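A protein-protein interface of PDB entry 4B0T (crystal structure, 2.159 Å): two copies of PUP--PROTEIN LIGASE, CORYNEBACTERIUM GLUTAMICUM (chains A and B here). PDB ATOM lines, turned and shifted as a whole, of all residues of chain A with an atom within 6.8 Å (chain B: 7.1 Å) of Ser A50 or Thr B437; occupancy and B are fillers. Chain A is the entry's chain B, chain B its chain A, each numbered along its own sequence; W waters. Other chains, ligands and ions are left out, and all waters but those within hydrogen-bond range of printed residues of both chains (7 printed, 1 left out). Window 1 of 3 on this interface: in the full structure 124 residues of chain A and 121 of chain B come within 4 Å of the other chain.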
ATOM      1  N   VAL A  45     -16.305 -35.569  32.518  1.00  0.00           N
ATOM      2  CA  VAL A  45     -15.232 -34.602  32.676  1.00  0.00           C
ATOM      3  C   VAL A  45     -13.884 -35.228  32.274  1.00  0.00           C
ATOM      4  O   VAL A  45     -13.154 -34.691  31.440  1.00  0.00           O
ATOM      5  CB  VAL A  45     -15.177 -34.072  34.133  1.00  0.00           C
ATOM      6  CG1 VAL A  45     -13.901 -33.277  34.385  1.00  0.00           C
ATOM      7  CG2 VAL A  45     -16.419 -33.219  34.443  1.00  0.00           C
ATOM      8  N   TYR A  48     -14.030 -36.264  28.239  1.00  0.00           N
ATOM      9  CA  TYR A  48     -14.287 -35.251  27.217  1.00  0.00           C
ATOM     10  C   TYR A  48     -13.890 -33.799  27.463  1.00  0.00           C
ATOM     11  O   TYR A  48     -13.979 -32.980  26.549  1.00  0.00           O
ATOM     12  CB  TYR A  48     -15.761 -35.348  26.792  1.00  0.00           C
ATOM     13  CG  TYR A  48     -16.059 -36.660  26.096  1.00  0.00           C
ATOM     14  CD1 TYR A  48     -15.499 -36.937  24.861  1.00  0.00           C
ATOM     15  CD2 TYR A  48     -16.876 -37.619  26.673  1.00  0.00           C
ATOM     16  CE1 TYR A  48     -15.750 -38.136  24.202  1.00  0.00           C
ATOM     17  CE2 TYR A  48     -17.136 -38.828  26.019  1.00  0.00           C
ATOM     18  CZ  TYR A  48     -16.561 -39.070  24.782  1.00  0.00           C
ATOM     19  OH  TYR A  48     -16.792 -40.242  24.108  1.00  0.00           O
ATOM     20  N   SER A  49     -13.465 -33.455  28.674  1.00  0.00           N
ATOM     21  CA  SER A  49     -13.129 -32.056  28.924  1.00  0.00           C
ATOM     22  C   SER A  49     -11.851 -31.697  28.179  1.00  0.00           C
ATOM     23  O   SER A  49     -11.030 -32.562  27.912  1.00  0.00           O
ATOM     24  CB  SER A  49     -12.966 -31.748  30.422  1.00  0.00           C
ATOM     25  OG  SER A  49     -11.821 -32.397  30.966  1.00  0.00           O
ATOM     26  N   SER A  50     -11.704 -30.420  27.848  1.00  0.00           N
ATOM     27  CA  SER A  50     -10.515 -29.928  27.179  1.00  0.00           C
ATOM     28  C   SER A  50      -9.267 -30.217  28.018  1.00  0.00           C
ATOM     29  O   SER A  50      -9.227 -29.919  29.210  1.00  0.00           O
ATOM     30  CB  SER A  50     -10.647 -28.417  26.935  1.00  0.00           C
ATOM     31  OG  SER A  50      -9.538 -27.914  26.206  1.00  0.00           O
ATOM     32  N   SER A  51      -8.253 -30.790  27.378  1.00  0.00           N
ATOM     33  CA  SER A  51      -6.975 -31.096  28.026  1.00  0.00           C
ATOM     34  C   SER A  51      -6.061 -29.878  28.262  1.00  0.00           C
ATOM     35  O   SER A  51      -5.062 -29.998  28.979  1.00  0.00           O
ATOM     36  CB  SER A  51      -6.208 -32.167  27.227  1.00  0.00           C
ATOM     37  OG  SER A  51      -6.886 -33.408  27.257  1.00  0.00           O
ATOM     38  N   ASN A  52      -6.402 -28.716  27.696  1.00  0.00           N
ATOM     39  CA  ASN A  52      -5.654 -27.489  28.029  1.00  0.00           C
ATOM     40  C   ASN A  52      -6.260 -26.786  29.233  1.00  0.00           C
ATOM     41  O   ASN A  52      -7.333 -26.192  29.128  1.00  0.00           O
ATOM     42  CB  ASN A  52      -5.660 -26.487  26.865  1.00  0.00           C
ATOM     43  CG  ASN A  52      -4.768 -26.901  25.731  1.00  0.00           C
ATOM     44  OD1 ASN A  52      -3.719 -27.504  25.940  1.00  0.00           O
ATOM     45  ND2 ASN A  52      -5.177 -26.570  24.510  1.00  0.00           N
ATOM     46  N   ILE A  53      -5.542 -26.805  30.351  1.00  0.00           N
ATOM     47  CA  ILE A  53      -6.079 -26.318  31.609  1.00  0.00           C
ATOM     48  C   ILE A  53      -5.362 -25.079  32.176  1.00  0.00           C
ATOM     49  O   ILE A  53      -4.190 -25.125  32.573  1.00  0.00           O
ATOM     50  CB  ILE A  53      -6.092 -27.441  32.643  1.00  0.00           C
ATOM     51  CG1 ILE A  53      -6.995 -28.587  32.156  1.00  0.00           C
ATOM     52  CG2 ILE A  53      -6.569 -26.916  33.972  1.00  0.00           C
ATOM     53  CD1 ILE A  53      -6.572 -29.913  32.654  1.00  0.00           C
ATOM     54  N   LEU A  61      -1.522 -25.938  31.978  1.00  0.00           N
ATOM     55  CA  LEU A  61      -1.095 -27.318  32.049  1.00  0.00           C
ATOM     56  C   LEU A  61      -1.795 -28.108  30.958  1.00  0.00           C
ATOM     57  O   LEU A  61      -3.000 -27.966  30.767  1.00  0.00           O
ATOM     58  CB  LEU A  61      -1.421 -27.920  33.424  1.00  0.00           C
ATOM     59  CG  LEU A  61      -0.507 -27.498  34.578  1.00  0.00           C
ATOM     60  CD1 LEU A  61      -1.160 -27.736  35.924  1.00  0.00           C
ATOM     61  CD2 LEU A  61       0.808 -28.275  34.490  1.00  0.00           C
ATOM     62  N   LEU A  63      -2.780 -31.752  30.323  1.00  0.00           N
ATOM     63  CA  LEU A  63      -2.937 -33.015  31.030  1.00  0.00           C
ATOM     64  C   LEU A  63      -3.858 -33.952  30.254  1.00  0.00           C
ATOM     65  O   LEU A  63      -5.062 -33.705  30.125  1.00  0.00           O
ATOM     66  CB  LEU A  63      -3.500 -32.785  32.434  1.00  0.00           C
ATOM     67  CG  LEU A  63      -2.762 -31.727  33.248  1.00  0.00           C
ATOM     68  CD1 LEU A  63      -3.356 -31.595  34.646  1.00  0.00           C
ATOM     69  CD2 LEU A  63      -1.268 -32.068  33.310  1.00  0.00           C
ATOM     70  N   VAL B  45      -7.770 -31.291  37.142  1.00  0.00           N
ATOM     71  CA  VAL B  45      -8.746 -31.385  36.059  1.00  0.00           C
ATOM     72  C   VAL B  45     -10.135 -31.002  36.552  1.00  0.00           C
ATOM     73  O   VAL B  45     -10.836 -30.244  35.902  1.00  0.00           O
ATOM     74  CB  VAL B  45      -8.823 -32.789  35.427  1.00  0.00           C
ATOM     75  CG1 VAL B  45     -10.112 -32.920  34.604  1.00  0.00           C
ATOM     76  CG2 VAL B  45      -7.602 -33.059  34.568  1.00  0.00           C
ATOM     77  N   TYR B  48      -9.909 -26.881  37.596  1.00  0.00           N
ATOM     78  CA  TYR B  48      -9.692 -25.903  36.531  1.00  0.00           C
ATOM     79  C   TYR B  48     -10.134 -26.157  35.080  1.00  0.00           C
ATOM     80  O   TYR B  48     -10.041 -25.247  34.241  1.00  0.00           O
ATOM     81  CB  TYR B  48      -8.227 -25.448  36.593  1.00  0.00           C
ATOM     82  CG  TYR B  48      -7.954 -24.775  37.916  1.00  0.00           C
ATOM     83  CD1 TYR B  48      -8.538 -23.554  38.219  1.00  0.00           C
ATOM     84  CD2 TYR B  48      -7.152 -25.375  38.875  1.00  0.00           C
ATOM     85  CE1 TYR B  48      -8.309 -22.937  39.423  1.00  0.00           C
ATOM     86  CE2 TYR B  48      -6.913 -24.762  40.088  1.00  0.00           C
ATOM     87  CZ  TYR B  48      -7.499 -23.548  40.357  1.00  0.00           C
ATOM     88  OH  TYR B  48      -7.274 -22.933  41.565  1.00  0.00           O
ATOM     89  N   SER B  49     -10.615 -27.357  34.765  1.00  0.00           N
ATOM     90  CA  SER B  49     -10.933 -27.646  33.383  1.00  0.00           C
ATOM     91  C   SER B  49     -12.165 -26.830  33.005  1.00  0.00           C
ATOM     92  O   SER B  49     -12.953 -26.494  33.868  1.00  0.00           O
ATOM     93  CB  SER B  49     -11.145 -29.148  33.135  1.00  0.00           C
ATOM     94  OG  SER B  49     -12.350 -29.631  33.711  1.00  0.00           O
ATOM     95  N   SER B  50     -12.315 -26.494  31.727  1.00  0.00           N
ATOM     96  CA  SER B  50     -13.516 -25.797  31.285  1.00  0.00           C
ATOM     97  C   SER B  50     -14.781 -26.636  31.533  1.00  0.00           C
ATOM     98  O   SER B  50     -14.810 -27.837  31.262  1.00  0.00           O
ATOM     99  CB  SER B  50     -13.414 -25.418  29.798  1.00  0.00           C
ATOM    100  OG  SER B  50     -14.686 -24.979  29.315  1.00  0.00           O
ATOM    101  N   ASN B  52     -17.535 -26.382  29.900  1.00  0.00           N
ATOM    102  CA  ASN B  52     -18.268 -26.652  28.671  1.00  0.00           C
ATOM    103  C   ASN B  52     -17.687 -27.890  27.984  1.00  0.00           C
ATOM    104  O   ASN B  52     -16.599 -27.848  27.423  1.00  0.00           O
ATOM    105  CB  ASN B  52     -18.182 -25.437  27.724  1.00  0.00           C
ATOM    106  CG  ASN B  52     -19.091 -24.290  28.163  1.00  0.00           C
ATOM    107  OD1 ASN B  52     -20.303 -24.465  28.308  1.00  0.00           O
ATOM    108  ND2 ASN B  52     -18.501 -23.129  28.421  1.00  0.00           N
ATOM    109  N   ILE B  53     -18.451 -28.974  27.988  1.00  0.00           N
ATOM    110  CA  ILE B  53     -17.957 -30.256  27.516  1.00  0.00           C
ATOM    111  C   ILE B  53     -18.678 -30.740  26.271  1.00  0.00           C
ATOM    112  O   ILE B  53     -19.870 -31.060  26.297  1.00  0.00           O
ATOM    113  CB  ILE B  53     -18.031 -31.313  28.621  1.00  0.00           C
ATOM    114  CG1 ILE B  53     -17.183 -30.855  29.813  1.00  0.00           C
ATOM    115  CG2 ILE B  53     -17.563 -32.687  28.099  1.00  0.00           C
ATOM    116  CD1 ILE B  53     -17.632 -31.441  31.108  1.00  0.00           C
ATOM    117  N   PHE B  54     -17.932 -30.806  25.177  1.00  0.00           N
ATOM    118  CA  PHE B  54     -18.492 -31.216  23.899  1.00  0.00           C
ATOM    119  C   PHE B  54     -18.316 -32.712  23.699  1.00  0.00           C
ATOM    120  O   PHE B  54     -17.232 -33.245  23.897  1.00  0.00           O
ATOM    121  CB  PHE B  54     -17.851 -30.419  22.756  1.00  0.00           C
ATOM    122  CG  PHE B  54     -18.404 -29.017  22.619  1.00  0.00           C
ATOM    123  CD1 PHE B  54     -17.868 -27.973  23.361  1.00  0.00           C
ATOM    124  CD2 PHE B  54     -19.493 -28.762  21.790  1.00  0.00           C
ATOM    125  CE1 PHE B  54     -18.391 -26.665  23.262  1.00  0.00           C
ATOM    126  CE2 PHE B  54     -20.026 -27.480  21.687  1.00  0.00           C
ATOM    127  CZ  PHE B  54     -19.471 -26.422  22.429  1.00  0.00           C
ATOM    128  N   ILE B 425     -14.736 -34.816  13.891  1.00  0.00           N
ATOM    129  CA  ILE B 425     -13.508 -34.449  14.571  1.00  0.00           C
ATOM    130  C   ILE B 425     -13.377 -35.161  15.920  1.00  0.00           C
ATOM    131  O   ILE B 425     -12.335 -35.715  16.255  1.00  0.00           O
ATOM    132  CB  ILE B 425     -13.448 -32.907  14.741  1.00  0.00           C
ATOM    133  CG1 ILE B 425     -13.137 -32.257  13.385  1.00  0.00           C
ATOM    134  CG2 ILE B 425     -12.453 -32.516  15.799  1.00  0.00           C
ATOM    135  CD1 ILE B 425     -13.306 -30.761  13.335  1.00  0.00           C
ATOM    136  N   LEU B 426     -14.457 -35.178  16.678  1.00  0.00           N
ATOM    137  CA  LEU B 426     -14.434 -35.778  18.003  1.00  0.00           C
ATOM    138  C   LEU B 426     -14.290 -37.293  17.940  1.00  0.00           C
ATOM    139  O   LEU B 426     -13.605 -37.886  18.759  1.00  0.00           O
ATOM    140  CB  LEU B 426     -15.681 -35.371  18.791  1.00  0.00           C
ATOM    141  CG  LEU B 426     -15.724 -33.884  19.180  1.00  0.00           C
ATOM    142  CD1 LEU B 426     -17.075 -33.549  19.820  1.00  0.00           C
ATOM    143  CD2 LEU B 426     -14.584 -33.582  20.152  1.00  0.00           C
ATOM    144  N   PRO B 435      -5.628 -35.344  21.614  1.00  0.00           N
ATOM    145  CA  PRO B 435      -6.408 -34.282  22.259  1.00  0.00           C
ATOM    146  C   PRO B 435      -6.871 -33.206  21.276  1.00  0.00           C
ATOM    147  O   PRO B 435      -6.089 -32.737  20.456  1.00  0.00           O
ATOM    148  CB  PRO B 435      -5.410 -33.685  23.255  1.00  0.00           C
ATOM    149  CG  PRO B 435      -4.088 -33.857  22.574  1.00  0.00           C
ATOM    150  CD  PRO B 435      -4.176 -35.148  21.793  1.00  0.00           C
ATOM    151  N   VAL B 436      -8.103 -32.747  21.428  1.00  0.00           N
ATOM    152  CA  VAL B 436      -8.655 -31.735  20.542  1.00  0.00           C
ATOM    153  C   VAL B 436      -9.534 -30.811  21.389  1.00  0.00           C
ATOM    154  O   VAL B 436     -10.046 -31.233  22.425  1.00  0.00           O
ATOM    155  CB  VAL B 436      -9.485 -32.419  19.429  1.00  0.00           C
ATOM    156  CG1 VAL B 436     -10.926 -32.620  19.888  1.00  0.00           C
ATOM    157  CG2 VAL B 436      -9.435 -31.632  18.166  1.00  0.00           C
ATOM    158  N   THR B 437      -9.683 -29.553  20.976  1.00  0.00           N
ATOM    159  CA  THR B 437     -10.525 -28.587  21.689  1.00  0.00           C
ATOM    160  C   THR B 437     -11.546 -27.964  20.737  1.00  0.00           C
ATOM    161  O   THR B 437     -11.170 -27.272  19.795  1.00  0.00           O
ATOM    162  CB  THR B 437      -9.681 -27.444  22.335  1.00  0.00           C
ATOM    163  OG1 THR B 437      -8.745 -27.997  23.273  1.00  0.00           O
ATOM    164  CG2 THR B 437     -10.591 -26.438  23.068  1.00  0.00           C
ATOM    165  N   VAL B 438     -12.834 -28.184  20.993  1.00  0.00           N
ATOM    166  CA  VAL B 438     -13.877 -27.669  20.102  1.00  0.00           C
ATOM    167  C   VAL B 438     -14.888 -26.764  20.802  1.00  0.00           C
ATOM    168  O   VAL B 438     -14.972 -26.737  22.014  1.00  0.00           O
ATOM    169  CB  VAL B 438     -14.637 -28.788  19.334  1.00  0.00           C
ATOM    170  CG1 VAL B 438     -13.667 -29.675  18.567  1.00  0.00           C
ATOM    171  CG2 VAL B 438     -15.495 -29.632  20.276  1.00  0.00           C
ATOM    172  N   ASP B 439     -15.639 -26.021  19.998  1.00  0.00           N
ATOM    173  CA  ASP B 439     -16.688 -25.129  20.458  1.00  0.00           C
ATOM    174  C   ASP B 439     -17.661 -25.076  19.282  1.00  0.00           C
ATOM    175  O   ASP B 439     -17.472 -25.804  18.314  1.00  0.00           O
ATOM    176  CB  ASP B 439     -16.099 -23.746  20.774  1.00  0.00           C
ATOM    177  CG  ASP B 439     -17.148 -22.752  21.256  1.00  0.00           C
ATOM    178  OD1 ASP B 439     -18.088 -23.164  21.964  1.00  0.00           O
ATOM    179  OD2 ASP B 439     -17.039 -21.554  20.914  1.00  0.00           O
ATOM    180  N   ARG B 442     -15.301 -22.744  16.617  1.00  0.00           N
ATOM    181  CA  ARG B 442     -13.859 -22.931  16.517  1.00  0.00           C
ATOM    182  C   ARG B 442     -13.460 -24.344  16.882  1.00  0.00           C
ATOM    183  O   ARG B 442     -13.878 -24.876  17.906  1.00  0.00           O
ATOM    184  CB  ARG B 442     -13.121 -21.915  17.394  1.00  0.00           C
ATOM    185  CG  ARG B 442     -11.614 -22.037  17.334  1.00  0.00           C
ATOM    186  CD  ARG B 442     -10.937 -20.840  17.984  1.00  0.00           C
ATOM    187  NE  ARG B 442     -11.258 -20.736  19.406  1.00  0.00           N
ATOM    188  CZ  ARG B 442     -10.802 -19.780  20.215  1.00  0.00           C
ATOM    189  NH1 ARG B 442      -9.999 -18.831  19.742  1.00  0.00           N
ATOM    190  NH2 ARG B 442     -11.152 -19.772  21.498  1.00  0.00           N
ATOM    191  N   HIS B 443     -12.650 -24.949  16.029  1.00  0.00           N
ATOM    192  CA  HIS B 443     -12.216 -26.317  16.222  1.00  0.00           C
ATOM    193  C   HIS B 443     -10.704 -26.361  16.097  1.00  0.00           C
ATOM    194  O   HIS B 443     -10.134 -25.867  15.125  1.00  0.00           O
ATOM    195  CB  HIS B 443     -12.893 -27.239  15.201  1.00  0.00           C
ATOM    196  CG  HIS B 443     -14.384 -27.267  15.320  1.00  0.00           C
ATOM    197  ND1 HIS B 443     -15.185 -26.207  14.944  1.00  0.00           N
ATOM    198  CD2 HIS B 443     -15.221 -28.216  15.810  1.00  0.00           C
ATOM    199  CE1 HIS B 443     -16.450 -26.508  15.184  1.00  0.00           C
ATOM    200  NE2 HIS B 443     -16.500 -27.724  15.705  1.00  0.00           N
ATOM    201  N   LYS B 444     -10.049 -26.948  17.086  1.00  0.00           N
ATOM    202  CA  LYS B 444      -8.609 -26.816  17.183  1.00  0.00           C
ATOM    203  C   LYS B 444      -7.962 -28.104  17.630  1.00  0.00           C
ATOM    204  O   LYS B 444      -8.455 -28.762  18.538  1.00  0.00           O
ATOM    205  CB  LYS B 444      -8.264 -25.669  18.152  1.00  0.00           C
ATOM    206  CG  LYS B 444      -6.803 -25.582  18.552  1.00  0.00           C
ATOM    207  CD  LYS B 444      -6.511 -24.298  19.351  1.00  0.00           C
ATOM    208  CE  LYS B 444      -7.471 -24.114  20.531  1.00  0.00           C
ATOM    209  NZ  LYS B 444      -7.014 -24.805  21.777  1.00  0.00           N
ATOM    210  N   VAL B 445      -6.868 -28.465  16.968  1.00  0.00           N
ATOM    211  CA  VAL B 445      -6.004 -29.556  17.396  1.00  0.00           C
ATOM    212  C   VAL B 445      -4.843 -28.903  18.093  1.00  0.00           C
ATOM    213  O   VAL B 445      -4.182 -28.032  17.538  1.00  0.00           O
ATOM    214  CB  VAL B 445      -5.457 -30.381  16.202  1.00  0.00           C
ATOM    215  CG1 VAL B 445      -4.445 -31.403  16.677  1.00  0.00           C
ATOM    216  CG2 VAL B 445      -6.590 -31.065  15.459  1.00  0.00           C
ATOM    217  N   ASN B 446      -4.598 -29.305  19.324  1.00  0.00           N
ATOM    218  CA  ASN B 446      -3.655 -28.585  20.153  1.00  0.00           C
ATOM    219  C   ASN B 446      -2.201 -28.954  19.913  1.00  0.00           C
ATOM    220  O   ASN B 446      -1.304 -28.203  20.294  1.00  0.00           O
ATOM    221  CB  ASN B 446      -4.037 -28.745  21.633  1.00  0.00           C
ATOM    222  CG  ASN B 446      -5.494 -28.390  21.895  1.00  0.00           C
ATOM    223  OD1 ASN B 446      -5.900 -27.239  21.728  1.00  0.00           O
ATOM    224  ND2 ASN B 446      -6.287 -29.379  22.306  1.00  0.00           N
ATOM    225  N   GLN B 451      -3.243 -26.550  15.028  1.00  0.00           N
ATOM    226  CA  GLN B 451      -4.056 -26.368  13.821  1.00  0.00           C
ATOM    227  C   GLN B 451      -5.503 -26.018  14.154  1.00  0.00           C
ATOM    228  O   GLN B 451      -6.202 -26.799  14.789  1.00  0.00           O
ATOM    229  CB  GLN B 451      -4.039 -27.640  12.977  1.00  0.00           C
ATOM    230  CG  GLN B 451      -2.665 -28.193  12.777  1.00  0.00           C
ATOM    231  CD  GLN B 451      -1.672 -27.096  12.472  1.00  0.00           C
ATOM    232  OE1 GLN B 451      -1.696 -26.502  11.390  1.00  0.00           O
ATOM    233  NE2 GLN B 451      -0.808 -26.798  13.437  1.00  0.00           N
HETATM  234  O   HOH W   1      -8.444 -31.745  24.760  1.00  0.00           O
HETATM  235  O   HOH W   2     -14.052 -28.783  28.594  1.00  0.00           O
HETATM  236  O   HOH W   3     -14.433 -33.106  23.804  1.00  0.00           O
HETATM  237  O   HOH W   4      -7.573 -24.163  24.928  1.00  0.00           O
HETATM  238  O   HOH W   5     -14.996 -30.187  25.647  1.00  0.00           O
HETATM  239  O   HOH W   6      -8.970 -24.464  31.660  1.00  0.00           O
HETATM  240  O   HOH W   7     -10.023 -27.243  30.065  1.00  0.00           O
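Water W3 lies within hydrogen-bond range of O of Tyr A48 and O of Phe B54.
Water W6 lies within hydrogen-bond range of O of Tyr B48 (2.9 Å) and O of Asn A52 (3.5 Å).
Water W7 lies within hydrogen-bond range of the backbone carbonyl oxygen of Ser A50, the backbone NH of Ser B50 and the backbone carbonyl oxygen of Asn A52.
Water W2 lies within hydrogen-bond range of the backbone carbonyl oxygen (O) of Ser B50, the backbone carbonyl oxygen (O) of Asn B52 and the backbone NH (N) of Ser A50.
Water W5 lies within hydrogen-bond range of the backbone NH of Phe B54 (3.0 Å), the backbone carbonyl oxygen of Tyr A48 (3.1 Å) and the backbone carbonyl oxygen of Asn B52 (3.3 Å).
Water W4 lies within hydrogen-bond range of the side-chain amino group of Lys B444 (3.3 Å) and the side-chain amide nitrogen of Asn A52 (3.4 Å).
Ser A50 touches just one residue of chain B: Thr B437 (3.0 Å).
Thr B437 touches one residue of chain A.
Printed residues of chain B within 4 Å of Val A45: Val B45 and Ile B53.
Printed residues of chain A within 4 Å of Phe B54: Tyr A48.
Of the printed residues of chain A, Val B45 touches Val A45 and Ile A53.
Printed residues of chain B within 4 Å of Ile A53: Val B45 and Tyr B48.
Printed residues of chain A within 4 Å of Asn B446: Asn A52.
His B443 touches none of the printed residues of chain A.
The nearest residue of chain A that does not touch Thr B437 is Asn A52 (4.04 Å).
The side-chain hydroxyl (OG1) of Thr B437 sits at hydrogen-bond distance from the side-chain hydroxyl (OG) of Ser A50 (3.0 Å).
The side-chain amide oxygen of Asn B446 is in hydrogen-bond range of the side-chain amide nitrogen of Asn A52.
Val B45 touches Val A45.
CG2 of Val A45 touches CD1 of Ile B53 (3.97 Å).
Tyr A48 touches Ile B53.
O of Phe B54 touches CB of Tyr A48 (3.9 Å).
Ser A49 touches Ser B49.
Asn A52 touches Lys B444.
Ile A53 touches Val B45 (CD1 to CG2, 3.8 Å).
Ile A53 touches Tyr B48 (CG2 to CB, 3.4 Å).
Val B45 touches its own counterpart, Val A45.
Val A45 touches Ile B53, and with the chains exchanged Ile A53 touches Val B45.
Tyr A48 touches Ile B53, and with the chains exchanged Ile A53 touches Tyr B48.
Ser B49 touches its own counterpart, Ser A49.
Positions printed for both chains: 45, 48, 49, 50, 52 and 53.
The backbone carbonyl oxygen (O) of Val B45 is in hydrogen-bond range of the side-chain hydroxyl (OG) of Ser B49, at 2.7 Å.
O of Lys B444 sits at hydrogen-bond distance from N of Thr B437 (2.8 Å).
The side-chain hydroxyl of Thr B437 lies within hydrogen-bond range of the side-chain amide nitrogen of Asn B446, at 3.0 Å.
NZ of Lys B444 sits at hydrogen-bond distance from OD1 of Asn B446, 2.7 Å away.
The backbone carbonyl oxygen of Val A45 sits at hydrogen-bond distance from the side-chain hydroxyl of Ser A49 (2.7 Å).
The backbone NH (N) of Ile A53 is in hydrogen-bond range of the backbone carbonyl oxygen (O) of Leu A61, at 2.8 Å.
Hydrophobic or aromatic side chains of chain A within 4 Å of the printed part of chain B: Val A45, Tyr A48 and Ile A53.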
